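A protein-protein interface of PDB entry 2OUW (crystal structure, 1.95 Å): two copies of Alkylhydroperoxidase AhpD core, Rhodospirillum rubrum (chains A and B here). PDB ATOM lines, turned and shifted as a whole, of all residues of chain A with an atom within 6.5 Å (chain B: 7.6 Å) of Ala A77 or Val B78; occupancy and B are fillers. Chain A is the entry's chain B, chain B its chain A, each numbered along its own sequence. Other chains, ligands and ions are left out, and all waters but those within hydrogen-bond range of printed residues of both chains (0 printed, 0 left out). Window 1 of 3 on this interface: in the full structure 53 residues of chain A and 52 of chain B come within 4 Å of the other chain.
Printed residues of chain A that touch a printed residue of chain B: Met A73, Ile A74, Tyr A75, Ala A77, Val A78, Ser A79, Ala A81, Asn A82, Ile A111, Ala A115, Ala A116 and Asn A119. Printed residues of chain B that touch a printed residue of chain A: Ile B74, Tyr B75, Ala B77, Val B78, Ser B79, Ala B81, Asn B82, Cys B87, Ala B115 and Asn B119. Hydrophobic or aromatic side chains of chain B that line the printed part of chain A: Ile B74, Tyr B75, Ala B77, Val B78, Ala B81 and Ala B115. Along chain B the printed residues that touch a printed residue of chain A span positions 74 to 119. Among the printed residues, 22 pairs touch across the chains. Among the printed residues, no Asp or Glu carboxylate lies within 4 Å of a Lys or Arg side-chain nitrogen of the other chain.
Glu A72 touches none of the printed residues of chain B. Ala A77 touches just these residues of chain B: Ile B74 and Val B78. Of the printed residues of chain B, Ala A116 touches Asn B82. Of the printed residues of chain A, Ile B74 touches Met A73 (3.8 Å), Ala A77 (3.8 Å) and Ile A111 (3.6 Å). Val B78 touches just these residues of chain A: Ala A77 (3.6 Å), Ala A115 (3.5 Å) and Asn A119 (3.8 Å). The nearest printed residue of chain A that does not touch Val B78 is Ile A112 (4.2 Å).
Among the printed residues, merely in contact across the chains: Met A73 with Ile B74, Ile A74 with Ala B77, Tyr A75 with Ala B115, Ala A77 with Ile B74, Ala A77 with Val B78, Val A78 with Ala B77, Val A78 with Ala B115, Val A78 with Asn B119, Ala A81 with Ala B81, Ala A81 with Asn B82, Asn A82 with Ala B81, Ile A111 with Ile B74, Ile A111 with Tyr B75, Ala A115 with Tyr B75, Ala A115 with Val B78, Ala A116 with Asn B82 and Asn A119 with Val B78.
The side-chain amide oxygen (OD1) of Asn B119 sits close to the backbone carbonyl oxygen (O) of Ala B115 (3.0 Å). The backbone carbonyl oxygen (O) of Tyr B75 is in hydrogen-bond range of the side-chain hydroxyl (OG) of Ser B79 (2.7 Å). The backbone carbonyl oxygen (O) of Ser B79 lies within hydrogen-bond range of the backbone NH (N) of Cys B84, at 3.1 Å. The backbone carbonyl oxygen (O) of Tyr A75 is in hydrogen-bond range of the side-chain hydroxyl (OG) of Ser A79. SG of Cys B84 forms a disulfide with SG of Cys B87, 2.1 Å away. The side-chain amide nitrogen (ND2) of Asn A119 lies close to the backbone carbonyl oxygen (O) of Ala A115, 3.2 Å away.
SG of Cys B87 lies within hydrogen-bond range of ND2 of Asn A119 (3.3 Å). The side-chain amide oxygen of Asn A119 lies within hydrogen-bond range of the side-chain amide nitrogen of Asn B82, at 3.0 Å. The side-chain amide oxygen of Asn B119 lies within hydrogen-bond range of the side-chain amide nitrogen of Asn A82 (3.0 Å). ND2 of Asn B119 lies within hydrogen-bond range of OG of Ser A79 (3.1 Å). The side-chain amide nitrogen (ND2) of Asn A119 is in hydrogen-bond range of the side-chain hydroxyl (OG) of Ser B79 (3.1 Å).
Met A73 touches Ile B74, but with the chains exchanged Ile A74 does not touch Met B73 (4.4 Å). Val A78 touches Asn B119, and with the chains exchanged Asn A119 touches Val B78. Ser A79 touches Asn B119, and with the chains exchanged Asn A119 touches Ser B79. Ala A81 touches Asn B82, and with the chains exchanged Asn A82 touches Ala B81. Positions printed for both chains: 72, 73, 74, 75, 76, 77, 78, 79, 80, 81, 82, 112, 115 and 119. Of the 22 pairs that touch across the chains among the printed residues, 17 have their exchanged pair printed and touching as well.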
ATOM      1  N   GLU A  72       5.720  25.919   2.303  1.00  0.00           N
ATOM      2  CA  GLU A  72       6.487  25.484   1.139  1.00  0.00           C
ATOM      3  C   GLU A  72       6.962  24.038   1.260  1.00  0.00           C
ATOM      4  O   GLU A  72       7.051  23.327   0.262  1.00  0.00           O
ATOM      5  CB  GLU A  72       7.707  26.372   0.884  1.00  0.00           C
ATOM      6  CG  GLU A  72       7.453  27.596   0.038  1.00  0.00           C
ATOM      7  CD  GLU A  72       6.805  27.328  -1.320  1.00  0.00           C
ATOM      8  OE1 GLU A  72       6.997  26.249  -1.927  1.00  0.00           O
ATOM      9  OE2 GLU A  72       6.098  28.238  -1.782  1.00  0.00           O
ATOM     10  N   MET A  73       7.268  23.587   2.471  1.00  0.00           N
ATOM     11  CA  MET A  73       7.756  22.208   2.625  1.00  0.00           C
ATOM     12  C   MET A  73       6.609  21.235   2.380  1.00  0.00           C
ATOM     13  O   MET A  73       6.784  20.204   1.750  1.00  0.00           O
ATOM     14  CB  MET A  73       8.372  22.017   4.004  1.00  0.00           C
ATOM     15  CG  MET A  73       9.606  22.880   4.199  1.00  0.00           C
ATOM     16  SD  MET A  73      10.518  22.608   5.890  1.00  0.00           S
ATOM     17  CE  MET A  73       9.069  21.985   7.032  1.00  0.00           C
ATOM     18  N   ILE A  74       5.420  21.587   2.849  1.00  0.00           N
ATOM     19  CA  ILE A  74       4.265  20.776   2.560  1.00  0.00           C
ATOM     20  C   ILE A  74       4.027  20.754   1.039  1.00  0.00           C
ATOM     21  O   ILE A  74       3.833  19.678   0.449  1.00  0.00           O
ATOM     22  CB  ILE A  74       3.026  21.288   3.269  1.00  0.00           C
ATOM     23  CG1 ILE A  74       3.127  21.052   4.775  1.00  0.00           C
ATOM     24  CG2 ILE A  74       1.795  20.576   2.755  1.00  0.00           C
ATOM     25  CD1 ILE A  74       2.120  21.867   5.592  1.00  0.00           C
ATOM     26  N   TYR A  75       4.080  21.922   0.402  1.00  0.00           N
ATOM     27  CA  TYR A  75       3.892  22.031  -1.062  1.00  0.00           C
ATOM     28  C   TYR A  75       4.892  21.181  -1.824  1.00  0.00           C
ATOM     29  O   TYR A  75       4.566  20.547  -2.837  1.00  0.00           O
ATOM     30  CB  TYR A  75       4.012  23.484  -1.507  1.00  0.00           C
ATOM     31  CG  TYR A  75       3.070  23.947  -2.617  1.00  0.00           C
ATOM     32  CD1 TYR A  75       3.194  23.475  -3.914  1.00  0.00           C
ATOM     33  CD2 TYR A  75       2.091  24.897  -2.370  1.00  0.00           C
ATOM     34  CE1 TYR A  75       2.357  23.945  -4.937  1.00  0.00           C
ATOM     35  CE2 TYR A  75       1.258  25.361  -3.379  1.00  0.00           C
ATOM     36  CZ  TYR A  75       1.399  24.884  -4.658  1.00  0.00           C
ATOM     37  OH  TYR A  75       0.574  25.344  -5.673  1.00  0.00           O
ATOM     38  N   LEU A  76       6.121  21.165  -1.330  1.00  0.00           N
ATOM     39  CA  LEU A  76       7.168  20.378  -1.938  1.00  0.00           C
ATOM     40  C   LEU A  76       6.921  18.897  -1.790  1.00  0.00           C
ATOM     41  O   LEU A  76       7.103  18.132  -2.739  1.00  0.00           O
ATOM     42  CB  LEU A  76       8.526  20.777  -1.368  1.00  0.00           C
ATOM     43  CG  LEU A  76       9.726  19.888  -1.687  1.00  0.00           C
ATOM     44  CD1 LEU A  76       9.969  19.822  -3.190  1.00  0.00           C
ATOM     45  CD2 LEU A  76      10.930  20.404  -0.955  1.00  0.00           C
ATOM     46  N   ALA A  77       6.499  18.461  -0.601  1.00  0.00           N
ATOM     47  CA  ALA A  77       6.195  17.045  -0.413  1.00  0.00           C
ATOM     48  C   ALA A  77       5.035  16.592  -1.305  1.00  0.00           C
ATOM     49  O   ALA A  77       5.072  15.503  -1.875  1.00  0.00           O
ATOM     50  CB  ALA A  77       5.884  16.754   1.027  1.00  0.00           C
ATOM     51  N   VAL A  78       3.997  17.433  -1.416  1.00  0.00           N
ATOM     52  CA  VAL A  78       2.852  17.119  -2.268  1.00  0.00           C
ATOM     53  C   VAL A  78       3.288  17.036  -3.705  1.00  0.00           C
ATOM     54  O   VAL A  78       2.943  16.091  -4.410  1.00  0.00           O
ATOM     55  CB  VAL A  78       1.685  18.109  -2.082  1.00  0.00           C
ATOM     56  CG1 VAL A  78       0.526  17.764  -3.001  1.00  0.00           C
ATOM     57  CG2 VAL A  78       1.202  18.020  -0.658  1.00  0.00           C
ATOM     58  N   SER A  79       4.102  18.009  -4.142  1.00  0.00           N
ATOM     59  CA  SER A  79       4.551  18.040  -5.521  1.00  0.00           C
ATOM     60  C   SER A  79       5.282  16.750  -5.873  1.00  0.00           C
ATOM     61  O   SER A  79       5.173  16.239  -6.992  1.00  0.00           O
ATOM     62  CB  SER A  79       5.405  19.295  -5.744  1.00  0.00           C
ATOM     63  OG  SER A  79       4.612  20.468  -5.475  1.00  0.00           O
ATOM     64  N   THR A  80       6.024  16.230  -4.898  1.00  0.00           N
ATOM     65  CA  THR A  80       6.832  15.033  -5.076  1.00  0.00           C
ATOM     66  C   THR A  80       5.965  13.826  -5.203  1.00  0.00           C
ATOM     67  O   THR A  80       6.187  13.006  -6.090  1.00  0.00           O
ATOM     68  CB  THR A  80       7.820  14.821  -3.894  1.00  0.00           C
ATOM     69  OG1 THR A  80       8.774  15.867  -3.898  1.00  0.00           O
ATOM     70  CG2 THR A  80       8.559  13.479  -3.999  1.00  0.00           C
ATOM     71  N   ALA A  81       4.962  13.719  -4.324  1.00  0.00           N
ATOM     72  CA  ALA A  81       4.096  12.568  -4.308  1.00  0.00           C
ATOM     73  C   ALA A  81       3.249  12.547  -5.579  1.00  0.00           C
ATOM     74  O   ALA A  81       2.902  11.474  -6.066  1.00  0.00           O
ATOM     75  CB  ALA A  81       3.185  12.592  -3.051  1.00  0.00           C
ATOM     76  N   ASN A  82       2.939  13.735  -6.117  1.00  0.00           N
ATOM     77  CA  ASN A  82       2.256  13.868  -7.418  1.00  0.00           C
ATOM     78  C   ASN A  82       3.178  13.722  -8.645  1.00  0.00           C
ATOM     79  O   ASN A  82       2.730  13.862  -9.787  1.00  0.00           O
ATOM     80  CB  ASN A  82       1.480  15.206  -7.448  1.00  0.00           C
ATOM     81  CG  ASN A  82       0.313  15.210  -6.468  1.00  0.00           C
ATOM     82  OD1 ASN A  82      -0.226  14.158  -6.186  1.00  0.00           O
ATOM     83  ND2 ASN A  82      -0.079  16.385  -5.957  1.00  0.00           N
ATOM     84  N   VAL A 108      13.006  16.710   5.338  1.00  0.00           N
ATOM     85  CA  VAL A 108      11.824  16.707   4.448  1.00  0.00           C
ATOM     86  C   VAL A 108      11.889  15.509   3.503  1.00  0.00           C
ATOM     87  O   VAL A 108      10.921  14.767   3.349  1.00  0.00           O
ATOM     88  CB  VAL A 108      11.700  18.019   3.622  1.00  0.00           C
ATOM     89  CG1 VAL A 108      10.583  17.899   2.599  1.00  0.00           C
ATOM     90  CG2 VAL A 108      11.452  19.208   4.519  1.00  0.00           C
ATOM     91  N   ILE A 111      11.225  12.221   5.317  1.00  0.00           N
ATOM     92  CA  ILE A 111       9.808  12.023   5.584  1.00  0.00           C
ATOM     93  C   ILE A 111       9.081  11.604   4.312  1.00  0.00           C
ATOM     94  O   ILE A 111       8.237  10.722   4.347  1.00  0.00           O
ATOM     95  CB  ILE A 111       9.176  13.294   6.141  1.00  0.00           C
ATOM     96  CG1 ILE A 111       9.774  13.617   7.513  1.00  0.00           C
ATOM     97  CG2 ILE A 111       7.654  13.142   6.244  1.00  0.00           C
ATOM     98  CD1 ILE A 111       9.441  14.990   7.994  1.00  0.00           C
ATOM     99  N   ILE A 112       9.406  12.246   3.193  1.00  0.00           N
ATOM    100  CA  ILE A 112       8.753  11.946   1.923  1.00  0.00           C
ATOM    101  C   ILE A 112       9.042  10.477   1.563  1.00  0.00           C
ATOM    102  O   ILE A 112       8.123   9.722   1.257  1.00  0.00           O
ATOM    103  CB  ILE A 112       9.227  12.894   0.811  1.00  0.00           C
ATOM    104  CG1 ILE A 112       8.716  14.330   1.035  1.00  0.00           C
ATOM    105  CG2 ILE A 112       8.803  12.384  -0.542  1.00  0.00           C
ATOM    106  CD1 ILE A 112       9.530  15.388   0.215  1.00  0.00           C
ATOM    107  N   GLY A 113      10.301  10.053   1.666  1.00  0.00           N
ATOM    108  CA  GLY A 113      10.648   8.638   1.424  1.00  0.00           C
ATOM    109  C   GLY A 113       9.945   7.644   2.348  1.00  0.00           C
ATOM    110  O   GLY A 113       9.402   6.626   1.900  1.00  0.00           O
ATOM    111  N   ALA A 115       7.203   8.101   4.231  1.00  0.00           N
ATOM    112  CA  ALA A 115       5.777   8.126   3.996  1.00  0.00           C
ATOM    113  C   ALA A 115       5.405   7.354   2.750  1.00  0.00           C
ATOM    114  O   ALA A 115       4.440   6.650   2.744  1.00  0.00           O
ATOM    115  CB  ALA A 115       5.268   9.575   3.898  1.00  0.00           C
ATOM    116  N   ALA A 116       6.180   7.481   1.681  1.00  0.00           N
ATOM    117  CA  ALA A 116       5.875   6.762   0.449  1.00  0.00           C
ATOM    118  C   ALA A 116       5.934   5.257   0.733  1.00  0.00           C
ATOM    119  O   ALA A 116       5.062   4.480   0.242  1.00  0.00           O
ATOM    120  CB  ALA A 116       6.868   7.163  -0.648  1.00  0.00           C
ATOM    121  N   ASN A 119       2.980   4.190   3.104  1.00  0.00           N
ATOM    122  CA  ASN A 119       1.728   4.288   2.338  1.00  0.00           C
ATOM    123  C   ASN A 119       1.566   3.041   1.432  1.00  0.00           C
ATOM    124  O   ASN A 119       0.490   2.430   1.359  1.00  0.00           O
ATOM    125  CB  ASN A 119       1.638   5.536   1.465  1.00  0.00           C
ATOM    126  CG  ASN A 119       1.600   6.870   2.239  1.00  0.00           C
ATOM    127  OD1 ASN A 119       1.754   7.909   1.610  1.00  0.00           O
ATOM    128  ND2 ASN A 119       1.392   6.857   3.550  1.00  0.00           N
ATOM    129  N   GLU B  72       4.817  15.558  11.130  1.00  0.00           N
ATOM    130  CA  GLU B  72       3.564  14.846  10.971  1.00  0.00           C
ATOM    131  C   GLU B  72       2.673  15.434   9.878  1.00  0.00           C
ATOM    132  O   GLU B  72       2.076  14.688   9.111  1.00  0.00           O
ATOM    133  CB  GLU B  72       2.831  14.775  12.307  1.00  0.00           C
ATOM    134  CG  GLU B  72       1.736  13.749  12.344  1.00  0.00           C
ATOM    135  CD  GLU B  72       2.205  12.337  12.087  1.00  0.00           C
ATOM    136  OE1 GLU B  72       3.134  11.865  12.777  1.00  0.00           O
ATOM    137  OE2 GLU B  72       1.613  11.690  11.205  1.00  0.00           O
ATOM    138  N   MET B  73       2.628  16.760   9.766  1.00  0.00           N
ATOM    139  CA  MET B  73       1.839  17.421   8.719  1.00  0.00           C
ATOM    140  C   MET B  73       2.381  17.198   7.316  1.00  0.00           C
ATOM    141  O   MET B  73       1.630  17.058   6.368  1.00  0.00           O
ATOM    142  CB  MET B  73       1.747  18.914   8.995  1.00  0.00           C
ATOM    143  CG  MET B  73       1.005  19.210  10.263  1.00  0.00           C
ATOM    144  SD  MET B  73       0.740  21.104  10.705  1.00  0.00           S
ATOM    145  CE  MET B  73       2.149  21.702   9.999  1.00  0.00           C
ATOM    146  N   ILE B  74       3.694  17.135   7.177  1.00  0.00           N
ATOM    147  CA  ILE B  74       4.297  16.728   5.900  1.00  0.00           C
ATOM    148  C   ILE B  74       3.923  15.281   5.602  1.00  0.00           C
ATOM    149  O   ILE B  74       3.580  14.942   4.474  1.00  0.00           O
ATOM    150  CB  ILE B  74       5.811  16.867   5.941  1.00  0.00           C
ATOM    151  CG1 ILE B  74       6.193  18.340   5.971  1.00  0.00           C
ATOM    152  CG2 ILE B  74       6.463  16.207   4.724  1.00  0.00           C
ATOM    153  CD1 ILE B  74       7.574  18.574   6.487  1.00  0.00           C
ATOM    154  N   TYR B  75       3.931  14.439   6.633  1.00  0.00           N
ATOM    155  CA  TYR B  75       3.586  13.015   6.474  1.00  0.00           C
ATOM    156  C   TYR B  75       2.127  12.825   6.030  1.00  0.00           C
ATOM    157  O   TYR B  75       1.822  11.961   5.223  1.00  0.00           O
ATOM    158  CB  TYR B  75       3.847  12.261   7.793  1.00  0.00           C
ATOM    159  CG  TYR B  75       4.304  10.810   7.669  1.00  0.00           C
ATOM    160  CD1 TYR B  75       3.436   9.808   7.223  1.00  0.00           C
ATOM    161  CD2 TYR B  75       5.595  10.436   8.040  1.00  0.00           C
ATOM    162  CE1 TYR B  75       3.853   8.458   7.141  1.00  0.00           C
ATOM    163  CE2 TYR B  75       6.026   9.111   7.947  1.00  0.00           C
ATOM    164  CZ  TYR B  75       5.142   8.119   7.504  1.00  0.00           C
ATOM    165  OH  TYR B  75       5.551   6.807   7.433  1.00  0.00           O
ATOM    166  N   LEU B  76       1.230  13.614   6.610  1.00  0.00           N
ATOM    167  CA  LEU B  76      -0.165  13.647   6.236  1.00  0.00           C
ATOM    168  C   LEU B  76      -0.371  14.092   4.797  1.00  0.00           C
ATOM    169  O   LEU B  76      -1.184  13.548   4.064  1.00  0.00           O
ATOM    170  CB  LEU B  76      -0.899  14.628   7.167  1.00  0.00           C
ATOM    171  CG  LEU B  76      -2.403  14.819   6.928  1.00  0.00           C
ATOM    172  CD1 LEU B  76      -3.117  13.471   6.825  1.00  0.00           C
ATOM    173  CD2 LEU B  76      -3.018  15.645   8.020  1.00  0.00           C
ATOM    174  N   ALA B  77       0.385  15.099   4.391  1.00  0.00           N
ATOM    175  CA  ALA B  77       0.259  15.635   3.053  1.00  0.00           C
ATOM    176  C   ALA B  77       0.646  14.574   2.032  1.00  0.00           C
ATOM    177  O   ALA B  77      -0.061  14.352   1.052  1.00  0.00           O
ATOM    178  CB  ALA B  77       1.132  16.861   2.907  1.00  0.00           C
ATOM    179  N   VAL B  78       1.773  13.911   2.270  1.00  0.00           N
ATOM    180  CA  VAL B  78       2.217  12.842   1.398  1.00  0.00           C
ATOM    181  C   VAL B  78       1.164  11.756   1.329  1.00  0.00           C
ATOM    182  O   VAL B  78       0.808  11.298   0.253  1.00  0.00           O
ATOM    183  CB  VAL B  78       3.614  12.290   1.837  1.00  0.00           C
ATOM    184  CG1 VAL B  78       3.990  11.049   1.050  1.00  0.00           C
ATOM    185  CG2 VAL B  78       4.666  13.369   1.623  1.00  0.00           C
ATOM    186  N   SER B  79       0.648  11.351   2.488  1.00  0.00           N
ATOM    187  CA  SER B  79      -0.289  10.247   2.549  1.00  0.00           C
ATOM    188  C   SER B  79      -1.522  10.523   1.690  1.00  0.00           C
ATOM    189  O   SER B  79      -2.049   9.608   1.021  1.00  0.00           O
ATOM    190  CB  SER B  79      -0.633   9.952   4.010  1.00  0.00           C
ATOM    191  OG  SER B  79       0.568   9.600   4.706  1.00  0.00           O
ATOM    192  N   THR B  80      -1.939  11.797   1.674  1.00  0.00           N
ATOM    193  CA  THR B  80      -3.096  12.247   0.882  1.00  0.00           C
ATOM    194  C   THR B  80      -2.782  12.235  -0.588  1.00  0.00           C
ATOM    195  O   THR B  80      -3.506  11.674  -1.379  1.00  0.00           O
ATOM    196  CB  THR B  80      -3.522  13.667   1.290  1.00  0.00           C
ATOM    197  OG1 THR B  80      -4.007  13.627   2.636  1.00  0.00           O
ATOM    198  CG2 THR B  80      -4.609  14.183   0.351  1.00  0.00           C
ATOM    199  N   ALA B  81      -1.664  12.828  -0.983  1.00  0.00           N
ATOM    200  CA  ALA B  81      -1.329  12.836  -2.374  1.00  0.00           C
ATOM    201  C   ALA B  81      -1.131  11.428  -2.926  1.00  0.00           C
ATOM    202  O   ALA B  81      -1.420  11.201  -4.102  1.00  0.00           O
ATOM    203  CB  ALA B  81      -0.053  13.677  -2.610  1.00  0.00           C
ATOM    204  N   ASN B  82      -0.616  10.495  -2.102  1.00  0.00           N
ATOM    205  CA  ASN B  82      -0.509   9.074  -2.502  1.00  0.00           C
ATOM    206  C   ASN B  82      -1.838   8.310  -2.410  1.00  0.00           C
ATOM    207  O   ASN B  82      -1.898   7.121  -2.708  1.00  0.00           O
ATOM    208  CB  ASN B  82       0.551   8.328  -1.677  1.00  0.00           C
ATOM    209  CG  ASN B  82       1.959   8.743  -2.011  1.00  0.00           C
ATOM    210  OD1 ASN B  82       2.256   9.146  -3.138  1.00  0.00           O
ATOM    211  ND2 ASN B  82       2.862   8.613  -1.034  1.00  0.00           N
ATOM    212  N   SER B  83      -2.890   8.986  -1.975  1.00  0.00           N
ATOM    213  CA  SER B  83      -4.241   8.444  -1.974  1.00  0.00           C
ATOM    214  C   SER B  83      -4.493   7.272  -1.007  1.00  0.00           C
ATOM    215  O   SER B  83      -5.417   6.490  -1.227  1.00  0.00           O
ATOM    216  CB  SER B  83      -4.670   8.066  -3.399  1.00  0.00           C
ATOM    217  OG  SER B  83      -6.089   7.976  -3.485  1.00  0.00           O
ATOM    218  N   CYS B  84      -3.698   7.174   0.067  1.00  0.00           N
ATOM    219  CA  CYS B  84      -3.851   6.094   1.059  1.00  0.00           C
ATOM    220  C   CYS B  84      -4.890   6.440   2.153  1.00  0.00           C
ATOM    221  O   CYS B  84      -4.612   7.214   3.068  1.00  0.00           O
ATOM    222  CB  CYS B  84      -2.494   5.787   1.715  1.00  0.00           C
ATOM    223  SG  CYS B  84      -2.623   4.558   3.017  1.00  0.00           S
ATOM    224  N   CYS B  87      -3.932   5.742   5.886  1.00  0.00           N
ATOM    225  CA  CYS B  87      -2.862   6.682   6.208  1.00  0.00           C
ATOM    226  C   CYS B  87      -3.365   8.113   6.439  1.00  0.00           C
ATOM    227  O   CYS B  87      -2.850   8.804   7.288  1.00  0.00           O
ATOM    228  CB  CYS B  87      -1.848   6.708   5.073  1.00  0.00           C
ATOM    229  SG  CYS B  87      -1.246   5.095   4.466  1.00  0.00           S
ATOM    230  N   ILE B 112      -2.724  21.336   0.291  1.00  0.00           N
ATOM    231  CA  ILE B 112      -2.806  20.068  -0.405  1.00  0.00           C
ATOM    232  C   ILE B 112      -3.676  20.219  -1.667  1.00  0.00           C
ATOM    233  O   ILE B 112      -3.315  19.746  -2.754  1.00  0.00           O
ATOM    234  CB  ILE B 112      -3.402  18.960   0.553  1.00  0.00           C
ATOM    235  CG1 ILE B 112      -2.374  18.471   1.586  1.00  0.00           C
ATOM    236  CG2 ILE B 112      -3.861  17.719  -0.233  1.00  0.00           C
ATOM    237  CD1 ILE B 112      -3.020  17.650   2.738  1.00  0.00           C
ATOM    238  N   ALA B 115      -1.744  22.646  -4.231  1.00  0.00           N
ATOM    239  CA  ALA B 115      -0.640  21.912  -4.860  1.00  0.00           C
ATOM    240  C   ALA B 115      -1.153  20.866  -5.818  1.00  0.00           C
ATOM    241  O   ALA B 115      -0.599  20.711  -6.882  1.00  0.00           O
ATOM    242  CB  ALA B 115       0.252  21.271  -3.821  1.00  0.00           C
ATOM    243  N   ASN B 119       0.195  21.355  -9.619  1.00  0.00           N
ATOM    244  CA  ASN B 119       0.913  20.197 -10.120  1.00  0.00           C
ATOM    245  C   ASN B 119       0.241  19.675 -11.414  1.00  0.00           C
ATOM    246  O   ASN B 119       0.921  19.410 -12.403  1.00  0.00           O
ATOM    247  CB  ASN B 119       0.915  19.065  -9.079  1.00  0.00           C
ATOM    248  CG  ASN B 119       1.756  19.369  -7.835  1.00  0.00           C
ATOM    249  OD1 ASN B 119       1.598  18.686  -6.832  1.00  0.00           O
ATOM    250  ND2 ASN B 119       2.673  20.354  -7.905  1.00  0.00           N
